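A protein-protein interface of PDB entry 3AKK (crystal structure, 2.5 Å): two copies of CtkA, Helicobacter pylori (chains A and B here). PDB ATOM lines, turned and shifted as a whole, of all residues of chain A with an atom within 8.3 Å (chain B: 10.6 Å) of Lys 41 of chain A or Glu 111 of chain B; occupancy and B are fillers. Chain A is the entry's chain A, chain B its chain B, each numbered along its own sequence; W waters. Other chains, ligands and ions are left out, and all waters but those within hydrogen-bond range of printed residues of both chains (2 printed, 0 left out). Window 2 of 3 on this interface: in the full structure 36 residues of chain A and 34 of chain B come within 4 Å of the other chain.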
ATOM      1  N   ASN A  21       5.253 -23.463   9.897  1.00  0.00           N
ATOM      2  CA  ASN A  21       6.373 -24.377   9.674  1.00  0.00           C
ATOM      3  C   ASN A  21       7.264 -24.045   8.470  1.00  0.00           C
ATOM      4  O   ASN A  21       7.444 -24.867   7.572  1.00  0.00           O
ATOM      5  CB  ASN A  21       5.872 -25.815   9.572  1.00  0.00           C
ATOM      6  CG  ASN A  21       5.216 -26.289  10.854  1.00  0.00           C
ATOM      7  OD1 ASN A  21       5.657 -25.930  11.952  1.00  0.00           O
ATOM      8  ND2 ASN A  21       4.153 -27.095  10.726  1.00  0.00           N
ATOM      9  N   GLY A  22       7.827 -22.845   8.451  1.00  0.00           N
ATOM     10  CA  GLY A  22       8.840 -22.534   7.465  1.00  0.00           C
ATOM     11  C   GLY A  22       8.343 -21.668   6.321  1.00  0.00           C
ATOM     12  O   GLY A  22       7.155 -21.379   6.192  1.00  0.00           O
ATOM     13  N   ASN A  23       9.271 -21.272   5.468  1.00  0.00           N
ATOM     14  CA  ASN A  23       8.984 -20.299   4.430  1.00  0.00           C
ATOM     15  C   ASN A  23       8.269 -20.888   3.223  1.00  0.00           C
ATOM     16  O   ASN A  23       8.251 -22.098   3.046  1.00  0.00           O
ATOM     17  CB  ASN A  23      10.286 -19.617   4.040  1.00  0.00           C
ATOM     18  CG  ASN A  23      10.991 -19.020   5.244  1.00  0.00           C
ATOM     19  OD1 ASN A  23      12.193 -18.779   5.227  1.00  0.00           O
ATOM     20  ND2 ASN A  23      10.234 -18.791   6.306  1.00  0.00           N
ATOM     21  N   PHE A  38       9.866 -24.447   2.361  1.00  0.00           N
ATOM     22  CA  PHE A  38      11.181 -24.704   2.924  1.00  0.00           C
ATOM     23  C   PHE A  38      10.958 -25.191   4.344  1.00  0.00           C
ATOM     24  O   PHE A  38      10.026 -24.758   5.017  1.00  0.00           O
ATOM     25  CB  PHE A  38      12.030 -23.424   2.925  1.00  0.00           C
ATOM     26  CG  PHE A  38      12.261 -22.837   1.545  1.00  0.00           C
ATOM     27  CD1 PHE A  38      11.221 -22.240   0.844  1.00  0.00           C
ATOM     28  CD2 PHE A  38      13.512 -22.889   0.953  1.00  0.00           C
ATOM     29  CE1 PHE A  38      11.422 -21.715  -0.410  1.00  0.00           C
ATOM     30  CE2 PHE A  38      13.719 -22.357  -0.298  1.00  0.00           C
ATOM     31  CZ  PHE A  38      12.672 -21.765  -0.982  1.00  0.00           C
ATOM     32  N   PRO A  39      11.781 -26.126   4.803  1.00  0.00           N
ATOM     33  CA  PRO A  39      11.669 -26.553   6.200  1.00  0.00           C
ATOM     34  C   PRO A  39      12.156 -25.446   7.126  1.00  0.00           C
ATOM     35  O   PRO A  39      13.007 -24.639   6.726  1.00  0.00           O
ATOM     36  CB  PRO A  39      12.636 -27.725   6.274  1.00  0.00           C
ATOM     37  CG  PRO A  39      13.648 -27.426   5.198  1.00  0.00           C
ATOM     38  CD  PRO A  39      12.843 -26.837   4.082  1.00  0.00           C
ATOM     39  N   PRO A  40      11.642 -25.403   8.359  1.00  0.00           N
ATOM     40  CA  PRO A  40      12.137 -24.337   9.231  1.00  0.00           C
ATOM     41  C   PRO A  40      13.571 -24.667   9.605  1.00  0.00           C
ATOM     42  O   PRO A  40      13.806 -25.760  10.101  1.00  0.00           O
ATOM     43  CB  PRO A  40      11.238 -24.446  10.471  1.00  0.00           C
ATOM     44  CG  PRO A  40      10.307 -25.639  10.226  1.00  0.00           C
ATOM     45  CD  PRO A  40      10.874 -26.420   9.094  1.00  0.00           C
ATOM     46  N   LYS A  41      14.520 -23.775   9.353  1.00  0.00           N
ATOM     47  CA  LYS A  41      15.905 -24.071   9.703  1.00  0.00           C
ATOM     48  C   LYS A  41      16.231 -23.406  11.032  1.00  0.00           C
ATOM     49  O   LYS A  41      16.209 -22.183  11.130  1.00  0.00           O
ATOM     50  CB  LYS A  41      16.848 -23.602   8.591  1.00  0.00           C
ATOM     51  CG  LYS A  41      18.340 -23.872   8.790  1.00  0.00           C
ATOM     52  CD  LYS A  41      19.077 -23.819   7.431  1.00  0.00           C
ATOM     53  CE  LYS A  41      20.593 -24.025   7.564  1.00  0.00           C
ATOM     54  NZ  LYS A  41      21.268 -22.987   8.416  1.00  0.00           N
ATOM     55  N   PRO A  42      16.519 -24.213  12.065  1.00  0.00           N
ATOM     56  CA  PRO A  42      16.822 -23.649  13.388  1.00  0.00           C
ATOM     57  C   PRO A  42      18.156 -22.912  13.327  1.00  0.00           C
ATOM     58  O   PRO A  42      18.896 -23.077  12.356  1.00  0.00           O
ATOM     59  CB  PRO A  42      16.948 -24.890  14.300  1.00  0.00           C
ATOM     60  CG  PRO A  42      16.580 -26.079  13.441  1.00  0.00           C
ATOM     61  CD  PRO A  42      16.770 -25.665  12.008  1.00  0.00           C
ATOM     62  N   SER A  43      18.462 -22.122  14.351  1.00  0.00           N
ATOM     63  CA  SER A  43      19.730 -21.406  14.401  1.00  0.00           C
ATOM     64  C   SER A  43      20.912 -22.373  14.370  1.00  0.00           C
ATOM     65  O   SER A  43      21.993 -22.021  13.929  1.00  0.00           O
ATOM     66  CB  SER A  43      19.794 -20.509  15.644  1.00  0.00           C
ATOM     67  OG  SER A  43      19.500 -21.238  16.819  1.00  0.00           O
ATOM     68  N   THR A  44      20.675 -23.605  14.806  1.00  0.00           N
ATOM     69  CA  THR A  44      21.720 -24.607  14.973  1.00  0.00           C
ATOM     70  C   THR A  44      21.072 -26.001  14.890  1.00  0.00           C
ATOM     71  O   THR A  44      19.963 -26.194  15.417  1.00  0.00           O
ATOM     72  CB  THR A  44      22.430 -24.407  16.346  1.00  0.00           C
ATOM     73  OG1 THR A  44      23.687 -23.752  16.150  1.00  0.00           O
ATOM     74  CG2 THR A  44      22.662 -25.703  17.061  1.00  0.00           C
ATOM     75  N   HIS A  45      21.735 -26.953  14.219  1.00  0.00           N
ATOM     76  CA  HIS A  45      21.217 -28.321  14.108  1.00  0.00           C
ATOM     77  C   HIS A  45      22.322 -29.377  14.224  1.00  0.00           C
ATOM     78  O   HIS A  45      22.493 -30.217  13.331  1.00  0.00           O
ATOM     79  CB  HIS A  45      20.439 -28.514  12.804  1.00  0.00           C
ATOM     80  CG  HIS A  45      21.236 -28.195  11.579  1.00  0.00           C
ATOM     81  ND1 HIS A  45      21.537 -26.901  11.203  1.00  0.00           N
ATOM     82  CD2 HIS A  45      21.793 -28.995  10.645  1.00  0.00           C
ATOM     83  CE1 HIS A  45      22.255 -26.921  10.095  1.00  0.00           C
ATOM     84  NE2 HIS A  45      22.419 -28.180   9.731  1.00  0.00           N
ATOM     85  N   MET A  48      21.208 -33.251  14.658  1.00  0.00           N
ATOM     86  CA  MET A  48      19.751 -33.363  14.556  1.00  0.00           C
ATOM     87  C   MET A  48      19.307 -33.072  13.124  1.00  0.00           C
ATOM     88  O   MET A  48      20.085 -32.535  12.323  1.00  0.00           O
ATOM     89  CB  MET A  48      19.030 -32.426  15.550  1.00  0.00           C
ATOM     90  CG  MET A  48      19.377 -30.944  15.398  1.00  0.00           C
ATOM     91  SD  MET A  48      18.362 -29.829  16.394  1.00  0.00           S
ATOM     92  CE  MET A  48      16.786 -29.869  15.514  1.00  0.00           C
ATOM     93  N   SER A  49      18.064 -33.437  12.810  1.00  0.00           N
ATOM     94  CA  SER A  49      17.457 -33.095  11.524  1.00  0.00           C
ATOM     95  C   SER A  49      16.351 -32.028  11.673  1.00  0.00           C
ATOM     96  O   SER A  49      15.626 -31.994  12.667  1.00  0.00           O
ATOM     97  CB  SER A  49      16.906 -34.348  10.833  1.00  0.00           C
ATOM     98  OG  SER A  49      17.934 -35.300  10.588  1.00  0.00           O
ATOM     99  N   TYR A  50      16.240 -31.149  10.684  1.00  0.00           N
ATOM    100  CA  TYR A  50      15.190 -30.133  10.677  1.00  0.00           C
ATOM    101  C   TYR A  50      14.404 -30.236   9.375  1.00  0.00           C
ATOM    102  O   TYR A  50      13.494 -29.442   9.109  1.00  0.00           O
ATOM    103  CB  TYR A  50      15.794 -28.725  10.812  1.00  0.00           C
ATOM    104  CG  TYR A  50      16.663 -28.301   9.636  1.00  0.00           C
ATOM    105  CD1 TYR A  50      16.117 -27.605   8.559  1.00  0.00           C
ATOM    106  CD2 TYR A  50      18.026 -28.591   9.606  1.00  0.00           C
ATOM    107  CE1 TYR A  50      16.898 -27.208   7.482  1.00  0.00           C
ATOM    108  CE2 TYR A  50      18.816 -28.204   8.533  1.00  0.00           C
ATOM    109  CZ  TYR A  50      18.246 -27.509   7.471  1.00  0.00           C
ATOM    110  OH  TYR A  50      19.017 -27.120   6.390  1.00  0.00           O
ATOM    111  N   THR A  51      14.743 -31.253   8.590  1.00  0.00           N
ATOM    112  CA  THR A  51      14.469 -31.238   7.161  1.00  0.00           C
ATOM    113  C   THR A  51      13.493 -32.327   6.686  1.00  0.00           C
ATOM    114  O   THR A  51      13.123 -32.388   5.512  1.00  0.00           O
ATOM    115  CB  THR A  51      15.809 -31.321   6.405  1.00  0.00           C
ATOM    116  OG1 THR A  51      15.705 -30.644   5.150  1.00  0.00           O
ATOM    117  CG2 THR A  51      16.230 -32.762   6.216  1.00  0.00           C
ATOM    118  N   LYS A  80      17.905 -22.591  -4.764  1.00  0.00           N
ATOM    119  CA  LYS A  80      19.147 -22.016  -4.249  1.00  0.00           C
ATOM    120  C   LYS A  80      19.819 -22.900  -3.189  1.00  0.00           C
ATOM    121  O   LYS A  80      20.044 -22.480  -2.062  1.00  0.00           O
ATOM    122  CB  LYS A  80      18.928 -20.570  -3.760  1.00  0.00           C
ATOM    123  CG  LYS A  80      18.615 -19.578  -4.904  1.00  0.00           C
ATOM    124  CD  LYS A  80      18.087 -18.211  -4.419  1.00  0.00           C
ATOM    125  CE  LYS A  80      17.827 -17.233  -5.602  1.00  0.00           C
ATOM    126  NZ  LYS A  80      17.299 -15.875  -5.192  1.00  0.00           N
ATOM    127  N   ASN A  81      20.119 -24.137  -3.562  1.00  0.00           N
ATOM    128  CA  ASN A  81      20.874 -25.041  -2.695  1.00  0.00           C
ATOM    129  C   ASN A  81      20.120 -25.499  -1.455  1.00  0.00           C
ATOM    130  O   ASN A  81      20.715 -26.048  -0.526  1.00  0.00           O
ATOM    131  CB  ASN A  81      22.201 -24.401  -2.287  1.00  0.00           C
ATOM    132  CG  ASN A  81      22.947 -23.835  -3.469  1.00  0.00           C
ATOM    133  OD1 ASN A  81      23.132 -24.524  -4.474  1.00  0.00           O
ATOM    134  ND2 ASN A  81      23.366 -22.577  -3.370  1.00  0.00           N
ATOM    135  N   LYS A  82      18.812 -25.277  -1.435  1.00  0.00           N
ATOM    136  CA  LYS A  82      18.007 -25.743  -0.321  1.00  0.00           C
ATOM    137  C   LYS A  82      16.967 -26.763  -0.748  1.00  0.00           C
ATOM    138  O   LYS A  82      16.304 -26.599  -1.789  1.00  0.00           O
ATOM    139  CB  LYS A  82      17.315 -24.571   0.368  1.00  0.00           C
ATOM    140  CG  LYS A  82      18.250 -23.703   1.184  1.00  0.00           C
ATOM    141  CD  LYS A  82      17.516 -22.507   1.746  1.00  0.00           C
ATOM    142  CE  LYS A  82      18.398 -21.270   1.685  1.00  0.00           C
ATOM    143  NZ  LYS A  82      18.929 -21.043   0.298  1.00  0.00           N
ATOM    144  N   LYS B 104       5.631 -12.289   4.866  1.00  0.00           N
ATOM    145  CA  LYS B 104       6.946 -12.472   5.468  1.00  0.00           C
ATOM    146  C   LYS B 104       7.441 -13.893   5.188  1.00  0.00           C
ATOM    147  O   LYS B 104       8.649 -14.123   5.044  1.00  0.00           O
ATOM    148  CB  LYS B 104       6.913 -12.180   6.977  1.00  0.00           C
ATOM    149  CG  LYS B 104       8.294 -12.166   7.654  1.00  0.00           C
ATOM    150  CD  LYS B 104       8.200 -11.764   9.128  1.00  0.00           C
ATOM    151  CE  LYS B 104       9.514 -11.989   9.866  1.00  0.00           C
ATOM    152  NZ  LYS B 104       9.838 -13.432  10.115  1.00  0.00           N
ATOM    153  N   ASN B 105       6.508 -14.840   5.093  1.00  0.00           N
ATOM    154  CA  ASN B 105       6.889 -16.212   4.764  1.00  0.00           C
ATOM    155  C   ASN B 105       7.728 -16.297   3.486  1.00  0.00           C
ATOM    156  O   ASN B 105       8.462 -17.267   3.304  1.00  0.00           O
ATOM    157  CB  ASN B 105       5.672 -17.147   4.684  1.00  0.00           C
ATOM    158  CG  ASN B 105       5.362 -17.789   6.005  1.00  0.00           C
ATOM    159  OD1 ASN B 105       6.227 -17.891   6.858  1.00  0.00           O
ATOM    160  ND2 ASN B 105       4.122 -18.211   6.191  1.00  0.00           N
ATOM    161  N   THR B 106       7.630 -15.278   2.627  1.00  0.00           N
ATOM    162  CA  THR B 106       8.411 -15.244   1.390  1.00  0.00           C
ATOM    163  C   THR B 106       9.878 -14.838   1.594  1.00  0.00           C
ATOM    164  O   THR B 106      10.713 -15.106   0.734  1.00  0.00           O
ATOM    165  CB  THR B 106       7.783 -14.345   0.267  1.00  0.00           C
ATOM    166  OG1 THR B 106       8.011 -12.957   0.550  1.00  0.00           O
ATOM    167  CG2 THR B 106       6.283 -14.611   0.072  1.00  0.00           C
ATOM    168  N   MET B 107      10.198 -14.199   2.716  1.00  0.00           N
ATOM    169  CA  MET B 107      11.571 -13.747   2.951  1.00  0.00           C
ATOM    170  C   MET B 107      12.498 -14.920   3.256  1.00  0.00           C
ATOM    171  O   MET B 107      12.873 -15.146   4.419  1.00  0.00           O
ATOM    172  CB  MET B 107      11.632 -12.710   4.081  1.00  0.00           C
ATOM    173  CG  MET B 107      10.870 -11.435   3.795  1.00  0.00           C
ATOM    174  SD  MET B 107      11.234 -10.796   2.157  1.00  0.00           S
ATOM    175  CE  MET B 107       9.645 -10.175   1.632  1.00  0.00           C
ATOM    176  N   ILE B 108      12.875 -15.659   2.212  1.00  0.00           N
ATOM    177  CA  ILE B 108      13.546 -16.950   2.394  1.00  0.00           C
ATOM    178  C   ILE B 108      14.996 -16.825   2.859  1.00  0.00           C
ATOM    179  O   ILE B 108      15.530 -17.747   3.465  1.00  0.00           O
ATOM    180  CB  ILE B 108      13.486 -17.847   1.122  1.00  0.00           C
ATOM    181  CG1 ILE B 108      14.263 -17.205  -0.036  1.00  0.00           C
ATOM    182  CG2 ILE B 108      12.042 -18.149   0.739  1.00  0.00           C
ATOM    183  CD1 ILE B 108      13.739 -17.553  -1.437  1.00  0.00           C
ATOM    184  N   GLU B 109      15.632 -15.694   2.587  1.00  0.00           N
ATOM    185  CA  GLU B 109      17.042 -15.541   2.931  1.00  0.00           C
ATOM    186  C   GLU B 109      17.214 -15.167   4.397  1.00  0.00           C
ATOM    187  O   GLU B 109      18.332 -15.104   4.895  1.00  0.00           O
ATOM    188  CB  GLU B 109      17.738 -14.529   2.011  1.00  0.00           C
ATOM    189  CG  GLU B 109      17.053 -13.174   1.901  1.00  0.00           C
ATOM    190  CD  GLU B 109      15.744 -13.229   1.120  1.00  0.00           C
ATOM    191  OE1 GLU B 109      15.502 -14.253   0.458  1.00  0.00           O
ATOM    192  OE2 GLU B 109      14.959 -12.251   1.158  1.00  0.00           O
ATOM    193  N   LEU B 110      16.100 -14.934   5.087  1.00  0.00           N
ATOM    194  CA  LEU B 110      16.133 -14.661   6.523  1.00  0.00           C
ATOM    195  C   LEU B 110      16.319 -15.935   7.350  1.00  0.00           C
ATOM    196  O   LEU B 110      16.965 -15.916   8.399  1.00  0.00           O
ATOM    197  CB  LEU B 110      14.872 -13.905   6.980  1.00  0.00           C
ATOM    198  CG  LEU B 110      14.826 -12.393   6.685  1.00  0.00           C
ATOM    199  CD1 LEU B 110      13.598 -11.688   7.297  1.00  0.00           C
ATOM    200  CD2 LEU B 110      16.117 -11.724   7.145  1.00  0.00           C
ATOM    201  N   GLU B 111      15.767 -17.043   6.876  1.00  0.00           N
ATOM    202  CA  GLU B 111      15.845 -18.292   7.629  1.00  0.00           C
ATOM    203  C   GLU B 111      15.146 -18.057   8.954  1.00  0.00           C
ATOM    204  O   GLU B 111      15.679 -18.356  10.024  1.00  0.00           O
ATOM    205  CB  GLU B 111      17.302 -18.748   7.839  1.00  0.00           C
ATOM    206  CG  GLU B 111      18.162 -18.730   6.551  1.00  0.00           C
ATOM    207  CD  GLU B 111      18.905 -20.043   6.257  1.00  0.00           C
ATOM    208  OE1 GLU B 111      19.688 -20.524   7.117  1.00  0.00           O
ATOM    209  OE2 GLU B 111      18.719 -20.579   5.141  1.00  0.00           O
ATOM    210  N   LYS B 112      13.954 -17.476   8.847  1.00  0.00           N
ATOM    211  CA  LYS B 112      13.059 -17.218   9.964  1.00  0.00           C
ATOM    212  C   LYS B 112      11.639 -17.426   9.429  1.00  0.00           C
ATOM    213  O   LYS B 112      11.365 -17.131   8.261  1.00  0.00           O
ATOM    214  CB  LYS B 112      13.202 -15.768  10.430  1.00  0.00           C
ATOM    215  CG  LYS B 112      14.603 -15.346  10.874  1.00  0.00           C
ATOM    216  CD  LYS B 112      14.877 -15.757  12.313  1.00  0.00           C
ATOM    217  CE  LYS B 112      16.228 -15.249  12.779  1.00  0.00           C
ATOM    218  NZ  LYS B 112      16.162 -13.968  13.557  1.00  0.00           N
ATOM    219  N   SER B 113      10.738 -17.929  10.263  1.00  0.00           N
ATOM    220  CA  SER B 113       9.332 -18.025   9.868  1.00  0.00           C
ATOM    221  C   SER B 113       8.681 -16.649   9.831  1.00  0.00           C
ATOM    222  O   SER B 113       9.031 -15.774  10.613  1.00  0.00           O
ATOM    223  CB  SER B 113       8.536 -18.955  10.799  1.00  0.00           C
ATOM    224  OG  SER B 113       8.525 -18.482  12.136  1.00  0.00           O
ATOM    225  N   GLY B 114       7.731 -16.467   8.924  1.00  0.00           N
ATOM    226  CA  GLY B 114       7.021 -15.209   8.800  1.00  0.00           C
ATOM    227  C   GLY B 114       6.128 -14.978   9.995  1.00  0.00           C
ATOM    228  O   GLY B 114       5.415 -13.999  10.052  1.00  0.00           O
ATOM    229  N   LYS B 115       6.176 -15.892  10.952  1.00  0.00           N
ATOM    230  CA  LYS B 115       5.387 -15.796  12.167  1.00  0.00           C
ATOM    231  C   LYS B 115       6.228 -15.148  13.251  1.00  0.00           C
ATOM    232  O   LYS B 115       5.702 -14.585  14.212  1.00  0.00           O
ATOM    233  CB  LYS B 115       4.967 -17.191  12.631  1.00  0.00           C
ATOM    234  CG  LYS B 115       4.064 -17.198  13.849  1.00  0.00           C
ATOM    235  CD  LYS B 115       4.316 -18.427  14.682  1.00  0.00           C
ATOM    236  CE  LYS B 115       3.329 -18.499  15.828  1.00  0.00           C
ATOM    237  NZ  LYS B 115       1.944 -18.830  15.354  1.00  0.00           N
ATOM    238  N   ASP B 116       7.542 -15.230  13.093  1.00  0.00           N
ATOM    239  CA  ASP B 116       8.454 -14.605  14.036  1.00  0.00           C
ATOM    240  C   ASP B 116       8.381 -13.069  13.936  1.00  0.00           C
ATOM    241  O   ASP B 116       8.354 -12.498  12.839  1.00  0.00           O
ATOM    242  CB  ASP B 116       9.869 -15.122  13.786  1.00  0.00           C
ATOM    243  CG  ASP B 116      10.881 -14.506  14.699  1.00  0.00           C
ATOM    244  OD1 ASP B 116      11.120 -15.059  15.790  1.00  0.00           O
ATOM    245  OD2 ASP B 116      11.456 -13.478  14.323  1.00  0.00           O
ATOM    246  N   ASN B 118      10.546 -10.606  15.092  1.00  0.00           N
ATOM    247  CA  ASN B 118      11.763  -9.830  15.271  1.00  0.00           C
ATOM    248  C   ASN B 118      11.635  -8.523  14.504  1.00  0.00           C
ATOM    249  O   ASN B 118      11.374  -8.539  13.305  1.00  0.00           O
ATOM    250  CB  ASN B 118      12.968 -10.610  14.763  1.00  0.00           C
ATOM    251  CG  ASN B 118      14.240  -9.793  14.793  1.00  0.00           C
ATOM    252  OD1 ASN B 118      14.592  -9.138  13.815  1.00  0.00           O
ATOM    253  ND2 ASN B 118      14.936  -9.824  15.920  1.00  0.00           N
ATOM    254  N   ASP B 121      13.761  -7.970  11.335  1.00  0.00           N
ATOM    255  CA  ASP B 121      13.297  -8.870  10.287  1.00  0.00           C
ATOM    256  C   ASP B 121      11.975  -8.393   9.705  1.00  0.00           C
ATOM    257  O   ASP B 121      11.752  -8.493   8.498  1.00  0.00           O
ATOM    258  CB  ASP B 121      13.122 -10.301  10.813  1.00  0.00           C
ATOM    259  CG  ASP B 121      14.448 -10.983  11.193  1.00  0.00           C
ATOM    260  OD1 ASP B 121      15.549 -10.452  10.886  1.00  0.00           O
ATOM    261  OD2 ASP B 121      14.366 -12.075  11.810  1.00  0.00           O
ATOM    262  N   TYR B 124      12.959  -5.620   7.473  1.00  0.00           N
ATOM    263  CA  TYR B 124      13.579  -6.203   6.299  1.00  0.00           C
ATOM    264  C   TYR B 124      12.502  -6.684   5.357  1.00  0.00           C
ATOM    265  O   TYR B 124      12.532  -6.357   4.170  1.00  0.00           O
ATOM    266  CB  TYR B 124      14.495  -7.358   6.674  1.00  0.00           C
ATOM    267  CG  TYR B 124      15.087  -8.059   5.469  1.00  0.00           C
ATOM    268  CD1 TYR B 124      16.398  -7.814   5.063  1.00  0.00           C
ATOM    269  CD2 TYR B 124      14.330  -8.962   4.727  1.00  0.00           C
ATOM    270  CE1 TYR B 124      16.933  -8.462   3.960  1.00  0.00           C
ATOM    271  CE2 TYR B 124      14.854  -9.607   3.625  1.00  0.00           C
ATOM    272  CZ  TYR B 124      16.153  -9.360   3.245  1.00  0.00           C
ATOM    273  OH  TYR B 124      16.667 -10.015   2.147  1.00  0.00           O
ATOM    274  N   ALA B 125      11.552  -7.454   5.888  1.00  0.00           N
ATOM    275  CA  ALA B 125      10.424  -7.933   5.095  1.00  0.00           C
ATOM    276  C   ALA B 125       9.678  -6.775   4.420  1.00  0.00           C
ATOM    277  O   ALA B 125       9.250  -6.884   3.265  1.00  0.00           O
ATOM    278  CB  ALA B 125       9.480  -8.736   5.957  1.00  0.00           C
HETATM  279  O   HOH W   1       6.675 -19.863   8.585  1.00  0.00           O
HETATM  280  O   HOH W   2      14.308 -20.524   3.932  1.00  0.00           O
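NZ of Lys 41 of chain A is in salt-bridge range of OE1 of Glu 111 of chain B (3.2 Å). O of Lys 112 of chain B sits at hydrogen-bond distance from ND2 of Asn 23 of chain A, at 2.8 Å.
The backbone carbonyl oxygen (O) of Ser 113 of chain B sits at hydrogen-bond distance from the side-chain amino group (NZ) of Lys 104 of chain B (2.5 Å). The side-chain amino group of Lys 82 of chain A is in hydrogen-bond range of the backbone carbonyl oxygen of Lys 80 of chain A (3.0 Å). The side-chain amino group (NZ) of Lys 112 of chain B is in salt-bridge range of the side-chain carboxylate (OD2) of Asp 121 of chain B. The side-chain amide oxygen (OD1) of Asn 105 of chain B lies within hydrogen-bond range of the backbone NH (N) of Gly 114 of chain B. O of Asn 23 of chain A is in hydrogen-bond range of N of Phe 38 of chain A (2.9 Å).
Among the printed residues, merely in contact across the chains: Gly 22 of chain A with Asn 105 of chain B (3.7 Å), Asn 23 of chain A with Asn 105 of chain B (3.1 Å), Asn 23 of chain A with Met 107 of chain B (3.8 Å), Asn 23 of chain A with Ile 108 of chain B (3.6 Å), Asn 23 of chain A with Ser 113 of chain B (3.8 Å), Phe 38 of chain A with Ile 108 of chain B (3.8 Å) and Lys 82 of chain A with Glu 111 of chain B (3.5 Å).
Lys 41 of chain A touches just one residue of chain B: Glu 111 (3.2 Å). Glu 111 of chain B touches just these residues of chain A: Lys 41 and Lys 82. No residue of chain B comes within 4 Å of Pro 39 of chain A. No residue of chain B comes within 4 Å of Pro 40 of chain A. Of the printed residues of chain A, Lys 112 of chain B touches Asn 23. Of the printed residues of chain A, Met 107 of chain B touches Asn 23 (3.8 Å). Printed residues of chain A within 4 Å of Asn 105 of chain B: Gly 22 (3.7 Å) and Asn 23 (3.1 Å). Thr 51 of chain A touches none of the printed residues of chain B. The nearest residue of chain B that does not touch Lys 41 of chain A is Lys 112 of chain B (5.7 Å). The nearest printed residue of chain B that does not touch Gly 22 of chain A is Ser 113 of chain B (4.6 Å).
Of the 17 printed residues of chain B, 6 touch a printed residue of chain A. Of the 18 printed residues of chain A, 5 touch a printed residue of chain B. Hydrophobic or aromatic side chains of chain A that line the printed part of chain B: Phe 38. Along chain A the printed residues that touch a printed residue of chain B span positions 22 to 82.
No position is printed for both chains.
Water W1 bridges OD1 of Asn 105 of chain B (2.7 Å) and O of Gly 22 of chain A (2.9 Å). Water W2 bridges OD1 of Asn 23 of chain A (3.0 Å) and O of Ile 108 of chain B (3.1 Å).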
